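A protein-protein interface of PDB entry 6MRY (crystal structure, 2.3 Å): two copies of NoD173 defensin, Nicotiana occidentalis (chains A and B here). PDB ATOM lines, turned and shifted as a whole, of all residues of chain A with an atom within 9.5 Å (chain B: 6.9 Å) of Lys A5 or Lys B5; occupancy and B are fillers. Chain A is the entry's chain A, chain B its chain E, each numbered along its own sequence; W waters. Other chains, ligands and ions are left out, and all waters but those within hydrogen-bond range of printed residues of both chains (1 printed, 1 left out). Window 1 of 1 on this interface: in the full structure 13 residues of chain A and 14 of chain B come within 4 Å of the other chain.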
ATOM      1  N   ALA A   1      15.033  -1.565 -21.215  1.00  0.00           N
ATOM      2  CA  ALA A   1      15.976  -2.551 -20.693  1.00  0.00           C
ATOM      3  C   ALA A   1      15.231  -3.640 -19.929  1.00  0.00           C
ATOM      4  O   ALA A   1      14.359  -4.320 -20.482  1.00  0.00           O
ATOM      5  CB  ALA A   1      17.002  -1.879 -19.800  1.00  0.00           C
ATOM      6  N   ARG A   2      15.585  -3.816 -18.658  1.00  0.00           N
ATOM      7  CA  ARG A   2      14.722  -4.538 -17.724  1.00  0.00           C
ATOM      8  C   ARG A   2      13.585  -3.595 -17.357  1.00  0.00           C
ATOM      9  O   ARG A   2      13.678  -2.791 -16.421  1.00  0.00           O
ATOM     10  CB  ARG A   2      15.484  -4.999 -16.487  1.00  0.00           C
ATOM     11  CG  ARG A   2      14.855  -6.219 -15.799  1.00  0.00           C
ATOM     12  CD  ARG A   2      14.952  -7.444 -16.708  1.00  0.00           C
ATOM     13  NE  ARG A   2      14.105  -8.554 -16.287  1.00  0.00           N
ATOM     14  CZ  ARG A   2      14.495  -9.511 -15.447  1.00  0.00           C
ATOM     15  NH1 ARG A   2      15.718  -9.490 -14.931  1.00  0.00           N
ATOM     16  NH2 ARG A   2      13.665 -10.496 -15.123  1.00  0.00           N
ATOM     17  N   GLN A   3      12.515  -3.673 -18.141  1.00  0.00           N
ATOM     18  CA  GLN A   3      11.281  -2.980 -17.811  1.00  0.00           C
ATOM     19  C   GLN A   3      10.701  -3.541 -16.519  1.00  0.00           C
ATOM     20  O   GLN A   3      10.542  -4.756 -16.375  1.00  0.00           O
ATOM     21  CB  GLN A   3      10.273  -3.142 -18.949  1.00  0.00           C
ATOM     22  CG  GLN A   3       9.296  -1.990 -19.101  1.00  0.00           C
ATOM     23  CD  GLN A   3       9.742  -1.007 -20.172  1.00  0.00           C
ATOM     24  OE1 GLN A   3      10.917  -0.618 -20.213  1.00  0.00           O
ATOM     25  NE2 GLN A   3       8.809  -0.592 -21.037  1.00  0.00           N
ATOM     26  N   CYS A   4      10.390  -2.655 -15.578  1.00  0.00           N
ATOM     27  CA  CYS A   4       9.577  -3.003 -14.435  1.00  0.00           C
ATOM     28  C   CYS A   4       8.234  -2.301 -14.523  1.00  0.00           C
ATOM     29  O   CYS A   4       8.129  -1.178 -15.035  1.00  0.00           O
ATOM     30  CB  CYS A   4      10.257  -2.622 -13.132  1.00  0.00           C
ATOM     31  SG  CYS A   4      11.288  -3.935 -12.508  1.00  0.00           S
ATOM     32  N   LYS A   5       7.225  -2.970 -13.965  1.00  0.00           N
ATOM     33  CA  LYS A   5       5.831  -2.577 -14.057  1.00  0.00           C
ATOM     34  C   LYS A   5       5.239  -2.433 -12.663  1.00  0.00           C
ATOM     35  O   LYS A   5       5.491  -3.256 -11.772  1.00  0.00           O
ATOM     36  CB  LYS A   5       5.019  -3.610 -14.848  1.00  0.00           C
ATOM     37  CG  LYS A   5       5.053  -3.427 -16.337  1.00  0.00           C
ATOM     38  CD  LYS A   5       5.090  -4.752 -17.079  1.00  0.00           C
ATOM     39  CE  LYS A   5       6.308  -5.581 -16.699  1.00  0.00           C
ATOM     40  NZ  LYS A   5       7.583  -4.985 -17.177  1.00  0.00           N
ATOM     41  N   ALA A   6       4.445  -1.388 -12.485  1.00  0.00           N
ATOM     42  CA  ALA A   6       3.708  -1.192 -11.245  1.00  0.00           C
ATOM     43  C   ALA A   6       2.357  -0.597 -11.599  1.00  0.00           C
ATOM     44  O   ALA A   6       2.286   0.333 -12.406  1.00  0.00           O
ATOM     45  CB  ALA A   6       4.476  -0.284 -10.276  1.00  0.00           C
ATOM     46  N   GLU A   7       1.291  -1.148 -11.024  1.00  0.00           N
ATOM     47  CA  GLU A   7      -0.045  -0.623 -11.284  1.00  0.00           C
ATOM     48  C   GLU A   7      -0.148   0.841 -10.854  1.00  0.00           C
ATOM     49  O   GLU A   7       0.317   1.222  -9.778  1.00  0.00           O
ATOM     50  CB  GLU A   7      -1.093  -1.464 -10.553  1.00  0.00           C
ATOM     51  CG  GLU A   7      -2.523  -1.189 -10.994  1.00  0.00           C
ATOM     52  CD  GLU A   7      -3.536  -2.145 -10.361  1.00  0.00           C
ATOM     53  OE1 GLU A   7      -3.139  -3.252  -9.942  1.00  0.00           O
ATOM     54  OE2 GLU A   7      -4.732  -1.790 -10.292  1.00  0.00           O
ATOM     55  N   SER A   8      -0.763   1.662 -11.712  1.00  0.00           N
ATOM     56  CA  SER A   8      -0.883   3.091 -11.452  1.00  0.00           C
ATOM     57  C   SER A   8      -1.558   3.372 -10.110  1.00  0.00           C
ATOM     58  O   SER A   8      -2.606   2.807  -9.784  1.00  0.00           O
ATOM     59  CB  SER A   8      -1.684   3.756 -12.555  1.00  0.00           C
ATOM     60  OG  SER A   8      -2.096   5.036 -12.134  1.00  0.00           O
ATOM     61  N   CYS A  21      -3.681   6.269 -19.399  1.00  0.00           N
ATOM     62  CA  CYS A  21      -2.823   5.485 -18.515  1.00  0.00           C
ATOM     63  C   CYS A  21      -1.394   6.004 -18.567  1.00  0.00           C
ATOM     64  O   CYS A  21      -0.744   6.183 -17.526  1.00  0.00           O
ATOM     65  CB  CYS A  21      -2.879   4.005 -18.902  1.00  0.00           C
ATOM     66  SG  CYS A  21      -1.712   2.981 -17.981  1.00  0.00           S
ATOM     67  N   CYS A  25       0.790   7.655 -15.601  1.00  0.00           N
ATOM     68  CA  CYS A  25       2.003   6.944 -15.210  1.00  0.00           C
ATOM     69  C   CYS A  25       3.199   7.861 -15.255  1.00  0.00           C
ATOM     70  O   CYS A  25       3.993   7.912 -14.304  1.00  0.00           O
ATOM     71  CB  CYS A  25       2.230   5.742 -16.107  1.00  0.00           C
ATOM     72  SG  CYS A  25       1.171   4.384 -15.680  1.00  0.00           S
ATOM     73  N   PHE A  30       6.876   7.681 -13.571  1.00  0.00           N
ATOM     74  CA  PHE A  30       7.336   6.558 -14.361  1.00  0.00           C
ATOM     75  C   PHE A  30       7.678   7.052 -15.766  1.00  0.00           C
ATOM     76  O   PHE A  30       7.475   8.219 -16.119  1.00  0.00           O
ATOM     77  CB  PHE A  30       6.274   5.463 -14.431  1.00  0.00           C
ATOM     78  CG  PHE A  30       6.230   4.585 -13.237  1.00  0.00           C
ATOM     79  CD1 PHE A  30       5.668   5.034 -12.057  1.00  0.00           C
ATOM     80  CD2 PHE A  30       6.731   3.298 -13.294  1.00  0.00           C
ATOM     81  CE1 PHE A  30       5.614   4.206 -10.938  1.00  0.00           C
ATOM     82  CE2 PHE A  30       6.678   2.470 -12.183  1.00  0.00           C
ATOM     83  CZ  PHE A  30       6.131   2.927 -11.004  1.00  0.00           C
ATOM     84  N   THR A  31       8.171   6.137 -16.598  1.00  0.00           N
ATOM     85  CA  THR A  31       8.540   6.485 -17.961  1.00  0.00           C
ATOM     86  C   THR A  31       7.370   6.339 -18.924  1.00  0.00           C
ATOM     87  O   THR A  31       7.215   7.163 -19.827  1.00  0.00           O
ATOM     88  CB  THR A  31       9.712   5.609 -18.417  1.00  0.00           C
ATOM     89  OG1 THR A  31      10.817   5.801 -17.528  1.00  0.00           O
ATOM     90  CG2 THR A  31      10.145   5.966 -19.834  1.00  0.00           C
ATOM     91  N   ASP A  32       6.535   5.311 -18.754  1.00  0.00           N
ATOM     92  CA  ASP A  32       5.412   5.098 -19.670  1.00  0.00           C
ATOM     93  C   ASP A  32       4.289   4.384 -18.922  1.00  0.00           C
ATOM     94  O   ASP A  32       4.406   4.084 -17.732  1.00  0.00           O
ATOM     95  CB  ASP A  32       5.868   4.307 -20.904  1.00  0.00           C
ATOM     96  CG  ASP A  32       4.937   4.477 -22.096  1.00  0.00           C
ATOM     97  OD1 ASP A  32       4.141   5.436 -22.122  1.00  0.00           O
ATOM     98  OD2 ASP A  32       4.982   3.627 -23.006  1.00  0.00           O
ATOM     99  N   GLY A  33       3.205   4.081 -19.634  1.00  0.00           N
ATOM    100  CA  GLY A  33       2.109   3.324 -19.057  1.00  0.00           C
ATOM    101  C   GLY A  33       1.305   2.642 -20.139  1.00  0.00           C
ATOM    102  O   GLY A  33       1.171   3.159 -21.252  1.00  0.00           O
ATOM    103  N   HIS A  34       0.757   1.476 -19.809  1.00  0.00           N
ATOM    104  CA  HIS A  34      -0.042   0.740 -20.779  1.00  0.00           C
ATOM    105  C   HIS A  34      -1.103  -0.096 -20.082  1.00  0.00           C
ATOM    106  O   HIS A  34      -0.950  -0.498 -18.928  1.00  0.00           O
ATOM    107  CB  HIS A  34       0.830  -0.169 -21.641  1.00  0.00           C
ATOM    108  CG  HIS A  34       1.597  -1.180 -20.850  1.00  0.00           C
ATOM    109  ND1 HIS A  34       1.170  -2.480 -20.688  1.00  0.00           N
ATOM    110  CD2 HIS A  34       2.753  -1.073 -20.155  1.00  0.00           C
ATOM    111  CE1 HIS A  34       2.041  -3.135 -19.940  1.00  0.00           C
ATOM    112  NE2 HIS A  34       3.010  -2.303 -19.603  1.00  0.00           N
ATOM    113  N   CYS A  35      -2.173  -0.371 -20.809  1.00  0.00           N
ATOM    114  CA  CYS A  35      -3.242  -1.198 -20.289  1.00  0.00           C
ATOM    115  C   CYS A  35      -2.821  -2.657 -20.321  1.00  0.00           C
ATOM    116  O   CYS A  35      -2.218  -3.120 -21.295  1.00  0.00           O
ATOM    117  CB  CYS A  35      -4.509  -0.975 -21.110  1.00  0.00           C
ATOM    118  SG  CYS A  35      -5.001   0.783 -21.187  1.00  0.00           S
ATOM    119  N   SER A  36      -3.085  -3.367 -19.221  1.00  0.00           N
ATOM    120  CA  SER A  36      -2.826  -4.801 -19.172  1.00  0.00           C
ATOM    121  C   SER A  36      -3.848  -5.521 -20.042  1.00  0.00           C
ATOM    122  O   SER A  36      -4.975  -5.060 -20.212  1.00  0.00           O
ATOM    123  CB  SER A  36      -2.872  -5.315 -17.727  1.00  0.00           C
ATOM    124  OG  SER A  36      -4.179  -5.258 -17.219  1.00  0.00           O
ATOM    125  N   LYS A  37      -3.447  -6.659 -20.604  1.00  0.00           N
ATOM    126  CA  LYS A  37      -4.207  -7.228 -21.713  1.00  0.00           C
ATOM    127  C   LYS A  37      -5.353  -8.119 -21.258  1.00  0.00           C
ATOM    128  O   LYS A  37      -6.272  -8.381 -22.045  1.00  0.00           O
ATOM    129  CB  LYS A  37      -3.296  -8.039 -22.638  1.00  0.00           C
ATOM    130  CG  LYS A  37      -2.071  -7.305 -23.122  1.00  0.00           C
ATOM    131  CD  LYS A  37      -2.450  -6.094 -23.946  1.00  0.00           C
ATOM    132  CE  LYS A  37      -1.221  -5.459 -24.572  1.00  0.00           C
ATOM    133  NZ  LYS A  37      -0.192  -5.062 -23.559  1.00  0.00           N
ATOM    134  N   ARG A  41      -5.874  -3.312 -16.546  1.00  0.00           N
ATOM    135  CA  ARG A  41      -5.303  -2.423 -15.552  1.00  0.00           C
ATOM    136  C   ARG A  41      -4.318  -1.465 -16.222  1.00  0.00           C
ATOM    137  O   ARG A  41      -3.733  -1.773 -17.263  1.00  0.00           O
ATOM    138  CB  ARG A  41      -4.600  -3.240 -14.464  1.00  0.00           C
ATOM    139  CG  ARG A  41      -5.472  -4.333 -13.877  1.00  0.00           C
ATOM    140  CD  ARG A  41      -4.775  -5.019 -12.719  1.00  0.00           C
ATOM    141  NE  ARG A  41      -3.703  -5.888 -13.189  1.00  0.00           N
ATOM    142  CZ  ARG A  41      -2.474  -5.915 -12.683  1.00  0.00           C
ATOM    143  NH1 ARG A  41      -1.572  -6.746 -13.199  1.00  0.00           N
ATOM    144  NH2 ARG A  41      -2.146  -5.122 -11.667  1.00  0.00           N
ATOM    145  N   CYS A  42      -4.144  -0.293 -15.621  1.00  0.00           N
ATOM    146  CA  CYS A  42      -3.143   0.662 -16.082  1.00  0.00           C
ATOM    147  C   CYS A  42      -1.833   0.340 -15.378  1.00  0.00           C
ATOM    148  O   CYS A  42      -1.714   0.530 -14.167  1.00  0.00           O
ATOM    149  CB  CYS A  42      -3.577   2.098 -15.795  1.00  0.00           C
ATOM    150  SG  CYS A  42      -2.238   3.311 -16.029  1.00  0.00           S
ATOM    151  N   LEU A  43      -0.853  -0.151 -16.120  1.00  0.00           N
ATOM    152  CA  LEU A  43       0.448  -0.508 -15.572  1.00  0.00           C
ATOM    153  C   LEU A  43       1.477   0.517 -16.025  1.00  0.00           C
ATOM    154  O   LEU A  43       1.665   0.715 -17.229  1.00  0.00           O
ATOM    155  CB  LEU A  43       0.870  -1.907 -16.023  1.00  0.00           C
ATOM    156  CG  LEU A  43      -0.098  -3.036 -15.690  1.00  0.00           C
ATOM    157  CD1 LEU A  43       0.485  -4.380 -16.141  1.00  0.00           C
ATOM    158  CD2 LEU A  43      -0.414  -3.031 -14.193  1.00  0.00           C
ATOM    159  N   CYS A  44       2.126   1.166 -15.063  1.00  0.00           N
ATOM    160  CA  CYS A  44       3.240   2.061 -15.307  1.00  0.00           C
ATOM    161  C   CYS A  44       4.524   1.268 -15.483  1.00  0.00           C
ATOM    162  O   CYS A  44       4.701   0.203 -14.889  1.00  0.00           O
ATOM    163  CB  CYS A  44       3.380   3.038 -14.146  1.00  0.00           C
ATOM    164  SG  CYS A  44       1.810   3.881 -13.811  1.00  0.00           S
ATOM    165  N   THR A  45       5.419   1.791 -16.327  1.00  0.00           N
ATOM    166  CA  THR A  45       6.678   1.130 -16.634  1.00  0.00           C
ATOM    167  C   THR A  45       7.841   2.098 -16.487  1.00  0.00           C
ATOM    168  O   THR A  45       7.753   3.269 -16.894  1.00  0.00           O
ATOM    169  CB  THR A  45       6.702   0.564 -18.054  1.00  0.00           C
ATOM    170  OG1 THR A  45       6.544   1.634 -19.001  1.00  0.00           O
ATOM    171  CG2 THR A  45       5.579  -0.463 -18.232  1.00  0.00           C
ATOM    172  N   LYS A  46       8.937   1.584 -15.924  1.00  0.00           N
ATOM    173  CA  LYS A  46      10.199   2.314 -15.833  1.00  0.00           C
ATOM    174  C   LYS A  46      11.346   1.313 -15.833  1.00  0.00           C
ATOM    175  O   LYS A  46      11.166   0.134 -15.527  1.00  0.00           O
ATOM    176  CB  LYS A  46      10.269   3.216 -14.585  1.00  0.00           C
ATOM    177  CG  LYS A  46      10.296   2.478 -13.235  1.00  0.00           C
ATOM    178  CD  LYS A  46      10.488   3.439 -12.056  1.00  0.00           C
ATOM    179  CE  LYS A  46       9.208   3.609 -11.247  1.00  0.00           C
ATOM    180  NZ  LYS A  46       9.218   4.779 -10.301  1.00  0.00           N
ATOM    181  N   ARG A  47      12.528   1.790 -16.207  1.00  0.00           N
ATOM    182  CA  ARG A  47      13.714   0.944 -16.186  1.00  0.00           C
ATOM    183  C   ARG A  47      14.004   0.520 -14.753  1.00  0.00           C
ATOM    184  O   ARG A  47      13.939   1.338 -13.834  1.00  0.00           O
ATOM    185  CB  ARG A  47      14.905   1.696 -16.786  1.00  0.00           C
ATOM    186  CG  ARG A  47      16.263   1.229 -16.292  1.00  0.00           C
ATOM    187  CD  ARG A  47      17.377   2.087 -16.879  1.00  0.00           C
ATOM    188  NE  ARG A  47      18.102   1.390 -17.943  1.00  0.00           N
ATOM    189  CZ  ARG A  47      17.921   1.601 -19.247  1.00  0.00           C
ATOM    190  NH1 ARG A  47      18.633   0.919 -20.137  1.00  0.00           N
ATOM    191  NH2 ARG A  47      17.035   2.493 -19.669  1.00  0.00           N
ATOM    192  N   CYS A  48      14.300  -0.756 -14.545  1.00  0.00           N
ATOM    193  CA  CYS A  48      14.612  -1.158 -13.178  1.00  0.00           C
ATOM    194  C   CYS A  48      15.848  -2.021 -13.063  1.00  0.00           C
ATOM    195  O   CYS A  48      16.518  -2.017 -12.036  1.00  0.00           O
ATOM    196  CB  CYS A  48      13.415  -1.885 -12.564  1.00  0.00           C
ATOM    197  SG  CYS A  48      13.078  -3.508 -13.267  1.00  0.00           S
ATOM    198  N   GLN B   3       6.425  -1.136  -5.143  1.00  0.00           N
ATOM    199  CA  GLN B   3       6.680  -2.533  -5.498  1.00  0.00           C
ATOM    200  C   GLN B   3       6.622  -2.693  -7.019  1.00  0.00           C
ATOM    201  O   GLN B   3       5.539  -2.650  -7.611  1.00  0.00           O
ATOM    202  CB  GLN B   3       5.658  -3.443  -4.817  1.00  0.00           C
ATOM    203  CG  GLN B   3       6.112  -4.878  -4.637  1.00  0.00           C
ATOM    204  CD  GLN B   3       7.309  -4.994  -3.701  1.00  0.00           C
ATOM    205  OE1 GLN B   3       7.389  -4.291  -2.691  1.00  0.00           O
ATOM    206  NE2 GLN B   3       8.243  -5.887  -4.029  1.00  0.00           N
ATOM    207  N   CYS B   4       7.778  -2.878  -7.656  1.00  0.00           N
ATOM    208  CA  CYS B   4       7.880  -3.054  -9.097  1.00  0.00           C
ATOM    209  C   CYS B   4       8.037  -4.528  -9.441  1.00  0.00           C
ATOM    210  O   CYS B   4       8.658  -5.297  -8.700  1.00  0.00           O
ATOM    211  CB  CYS B   4       9.072  -2.283  -9.668  1.00  0.00           C
ATOM    212  SG  CYS B   4       8.749  -0.565 -10.111  1.00  0.00           S
ATOM    213  N   LYS B   5       7.478  -4.911 -10.590  1.00  0.00           N
ATOM    214  CA  LYS B   5       7.483  -6.295 -11.033  1.00  0.00           C
ATOM    215  C   LYS B   5       8.093  -6.388 -12.428  1.00  0.00           C
ATOM    216  O   LYS B   5       8.012  -5.453 -13.227  1.00  0.00           O
ATOM    217  CB  LYS B   5       6.061  -6.884 -11.003  1.00  0.00           C
ATOM    218  CG  LYS B   5       5.259  -6.424  -9.782  1.00  0.00           C
ATOM    219  CD  LYS B   5       4.224  -7.432  -9.326  1.00  0.00           C
ATOM    220  CE  LYS B   5       3.406  -6.909  -8.130  1.00  0.00           C
ATOM    221  NZ  LYS B   5       4.170  -6.782  -6.839  1.00  0.00           N
ATOM    222  N   ALA B   6       8.746  -7.514 -12.686  1.00  0.00           N
ATOM    223  CA  ALA B   6       9.310  -7.839 -13.988  1.00  0.00           C
ATOM    224  C   ALA B   6       9.213  -9.340 -14.170  1.00  0.00           C
ATOM    225  O   ALA B   6       9.532 -10.087 -13.254  1.00  0.00           O
ATOM    226  CB  ALA B   6      10.770  -7.397 -14.103  1.00  0.00           C
ATOM    227  N   GLU B   7       8.770  -9.787 -15.332  1.00  0.00           N
ATOM    228  CA  GLU B   7       8.771 -11.222 -15.570  1.00  0.00           C
ATOM    229  C   GLU B   7      10.191 -11.786 -15.494  1.00  0.00           C
ATOM    230  O   GLU B   7      11.153 -11.169 -15.961  1.00  0.00           O
ATOM    231  CB  GLU B   7       8.135 -11.532 -16.919  1.00  0.00           C
ATOM    232  CG  GLU B   7       7.905 -13.027 -17.131  1.00  0.00           C
ATOM    233  CD  GLU B   7       7.096 -13.309 -18.384  1.00  0.00           C
ATOM    234  OE1 GLU B   7       6.681 -12.328 -19.042  1.00  0.00           O
ATOM    235  OE2 GLU B   7       6.870 -14.506 -18.698  1.00  0.00           O
ATOM    236  N   PHE B  30      16.383 -10.123  -7.501  1.00  0.00           N
ATOM    237  CA  PHE B  30      15.145  -9.512  -7.043  1.00  0.00           C
ATOM    238  C   PHE B  30      14.876  -9.899  -5.596  1.00  0.00           C
ATOM    239  O   PHE B  30      15.541 -10.763  -5.017  1.00  0.00           O
ATOM    240  CB  PHE B  30      13.963  -9.925  -7.917  1.00  0.00           C
ATOM    241  CG  PHE B  30      13.906  -9.206  -9.228  1.00  0.00           C
ATOM    242  CD1 PHE B  30      14.690  -9.629 -10.294  1.00  0.00           C
ATOM    243  CD2 PHE B  30      13.066  -8.126  -9.407  1.00  0.00           C
ATOM    244  CE1 PHE B  30      14.641  -8.978 -11.520  1.00  0.00           C
ATOM    245  CE2 PHE B  30      13.014  -7.470 -10.629  1.00  0.00           C
ATOM    246  CZ  PHE B  30      13.799  -7.893 -11.686  1.00  0.00           C
ATOM    247  N   HIS B  34       6.480 -14.228  -7.482  1.00  0.00           N
ATOM    248  CA  HIS B  34       5.171 -14.837  -7.281  1.00  0.00           C
ATOM    249  C   HIS B  34       4.539 -15.113  -8.634  1.00  0.00           C
ATOM    250  O   HIS B  34       4.901 -14.508  -9.647  1.00  0.00           O
ATOM    251  CB  HIS B  34       4.257 -13.950  -6.435  1.00  0.00           C
ATOM    252  CG  HIS B  34       3.969 -12.617  -7.050  1.00  0.00           C
ATOM    253  ND1 HIS B  34       2.971 -12.426  -7.984  1.00  0.00           N
ATOM    254  CD2 HIS B  34       4.539 -11.404  -6.855  1.00  0.00           C
ATOM    255  CE1 HIS B  34       2.945 -11.154  -8.343  1.00  0.00           C
ATOM    256  NE2 HIS B  34       3.887 -10.511  -7.670  1.00  0.00           N
ATOM    257  N   ARG B  41       2.384 -16.614 -15.053  1.00  0.00           N
ATOM    258  CA  ARG B  41       3.770 -16.263 -15.301  1.00  0.00           C
ATOM    259  C   ARG B  41       4.452 -15.997 -13.973  1.00  0.00           C
ATOM    260  O   ARG B  41       3.797 -15.697 -12.971  1.00  0.00           O
ATOM    261  CB  ARG B  41       3.904 -15.019 -16.182  1.00  0.00           C
ATOM    262  CG  ARG B  41       2.891 -14.858 -17.294  1.00  0.00           C
ATOM    263  CD  ARG B  41       3.115 -13.527 -18.038  1.00  0.00           C
ATOM    264  NE  ARG B  41       2.488 -12.392 -17.354  1.00  0.00           N
ATOM    265  CZ  ARG B  41       3.029 -11.181 -17.232  1.00  0.00           C
ATOM    266  NH1 ARG B  41       4.223 -10.906 -17.768  1.00  0.00           N
ATOM    267  NH2 ARG B  41       2.360 -10.233 -16.584  1.00  0.00           N
ATOM    268  N   LEU B  43       6.512 -13.611 -11.855  1.00  0.00           N
ATOM    269  CA  LEU B  43       6.847 -12.199 -11.745  1.00  0.00           C
ATOM    270  C   LEU B  43       7.833 -12.034 -10.605  1.00  0.00           C
ATOM    271  O   LEU B  43       7.586 -12.517  -9.500  1.00  0.00           O
ATOM    272  CB  LEU B  43       5.601 -11.355 -11.499  1.00  0.00           C
ATOM    273  CG  LEU B  43       4.587 -11.452 -12.634  1.00  0.00           C
ATOM    274  CD1 LEU B  43       3.413 -10.545 -12.343  1.00  0.00           C
ATOM    275  CD2 LEU B  43       5.248 -11.112 -13.992  1.00  0.00           C
ATOM    276  N   CYS B  44       8.954 -11.383 -10.884  1.00  0.00           N
ATOM    277  CA  CYS B  44       9.924 -10.993  -9.882  1.00  0.00           C
ATOM    278  C   CYS B  44       9.569  -9.604  -9.382  1.00  0.00           C
ATOM    279  O   CYS B  44       9.130  -8.754 -10.152  1.00  0.00           O
ATOM    280  CB  CYS B  44      11.337 -11.002 -10.474  1.00  0.00           C
ATOM    281  SG  CYS B  44      11.872 -12.616 -11.113  1.00  0.00           S
ATOM    282  N   THR B  45       9.752  -9.376  -8.090  1.00  0.00           N
ATOM    283  CA  THR B  45       9.356  -8.123  -7.468  1.00  0.00           C
ATOM    284  C   THR B  45      10.519  -7.559  -6.678  1.00  0.00           C
ATOM    285  O   THR B  45      11.295  -8.305  -6.064  1.00  0.00           O
ATOM    286  CB  THR B  45       8.182  -8.289  -6.506  1.00  0.00           C
ATOM    287  OG1 THR B  45       8.511  -9.309  -5.555  1.00  0.00           O
ATOM    288  CG2 THR B  45       6.913  -8.669  -7.238  1.00  0.00           C
ATOM    289  N   LYS B  46      10.593  -6.233  -6.665  1.00  0.00           N
ATOM    290  CA  LYS B  46      11.607  -5.522  -5.905  1.00  0.00           C
ATOM    291  C   LYS B  46      11.121  -4.105  -5.641  1.00  0.00           C
ATOM    292  O   LYS B  46      10.323  -3.549  -6.406  1.00  0.00           O
ATOM    293  CB  LYS B  46      12.947  -5.512  -6.644  1.00  0.00           C
ATOM    294  CG  LYS B  46      13.147  -4.315  -7.571  1.00  0.00           C
ATOM    295  CD  LYS B  46      14.205  -4.615  -8.618  1.00  0.00           C
ATOM    296  CE  LYS B  46      15.129  -3.435  -8.829  1.00  0.00           C
ATOM    297  NZ  LYS B  46      16.025  -3.662 -10.002  1.00  0.00           N
ATOM    298  N   CYS B  48      11.092  -0.261  -5.759  1.00  0.00           N
ATOM    299  CA  CYS B  48      11.514   0.623  -6.835  1.00  0.00           C
ATOM    300  C   CYS B  48      11.056   2.048  -6.567  1.00  0.00           C
ATOM    301  O   CYS B  48      10.934   2.848  -7.494  1.00  0.00           O
ATOM    302  CB  CYS B  48      10.963   0.146  -8.181  1.00  0.00           C
ATOM    303  SG  CYS B  48       9.189   0.433  -8.409  1.00  0.00           S
HETATM  304  O   HOH W   1       7.962  -7.979 -17.677  1.00  0.00           O
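The backbone carbonyl oxygen of Glu B7 lies within hydrogen-bond range of the guanidinium group of Arg A2 (2.7 Å).
The backbone carbonyl oxygen (O) of Lys B5 lies within hydrogen-bond range of the backbone NH (N) of Lys A5 (2.7 Å).
O of Cys A48 sits at hydrogen-bond distance from NZ of Lys B46 (2.7 Å).
The backbone carbonyl oxygen (O) of Lys B5 sits close to the side-chain sulfur (SG) of Cys A4, 3.7 Å away.
The backbone carbonyl oxygen of Arg A2 sits at hydrogen-bond distance from the backbone NH of Cys A48 (2.8 Å).
SG of Cys A4 forms a disulfide with SG of Cys A48 (2.0 Å).
The backbone carbonyl oxygen (O) of Ala A6 sits at hydrogen-bond distance from the backbone NH (N) of Cys A44.
The side-chain sulfur (SG) of Cys B4 is disulfide-bonded to the side-chain sulfur (SG) of Cys B48 (2.0 Å).
The side-chain carboxylate (OE1) of Glu B7 lies within salt-bridge range of the guanidinium group (NH1) of Arg B41 (3.1 Å).
The side-chain sulfur of Cys A25 is disulfide-bonded to the side-chain sulfur of Cys A44 (2.0 Å).
Among the printed residues, pairs that only touch across the chains: Arg A2 with Phe B30, Gln A3 with Ala B6, Cys A4 with Cys B4, Cys A4 with Ala B6, Lys A5 with Cys B4, Ala A6 with Gln B3 and Lys A46 with Cys B48.
Lys A5 touches two residues of chain B.
Of the printed residues of chain B, Lys A46 touches Cys B48 (3.8 Å).
Of chain A, only Cys A4 and Lys A5 come within 4 Å of Cys B4.
Lys B5 touches two residues of chain A.
Ala B6 touches just these residues of chain A: Gln A3 (3.5 Å) and Cys A4 (3.8 Å).
Of the printed residues of chain A, Glu B7 touches Arg A2 (2.7 Å).
Printed residues of chain A within 4 Å of Phe B30: Arg A2.
Hydrophobic or aromatic side chains of chain A within 4 Å of the printed part of chain B: Ala A6.
Hydrophobic or aromatic side chains of chain B that line the printed part of chain A: Ala B6 and Phe B30.
Cys A4 touches its own counterpart, Cys B4.
Cys A4 touches Ala B6, but with the chains exchanged Ala A6 does not touch Cys B4 (4.3 Å).
Lys A5 touches its own counterpart, Lys B5.
Lys A46 touches Cys B48, and with the chains exchanged Cys A48 touches Lys B46.
Positions printed for both chains: 3, 4, 5, 6, 7, 30, 34, 41, 43, 44, 45, 46 and 48.
Water W1 bridges the side-chain amino group (NZ) of Lys A5 and the backbone NH (N) of Glu B7.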
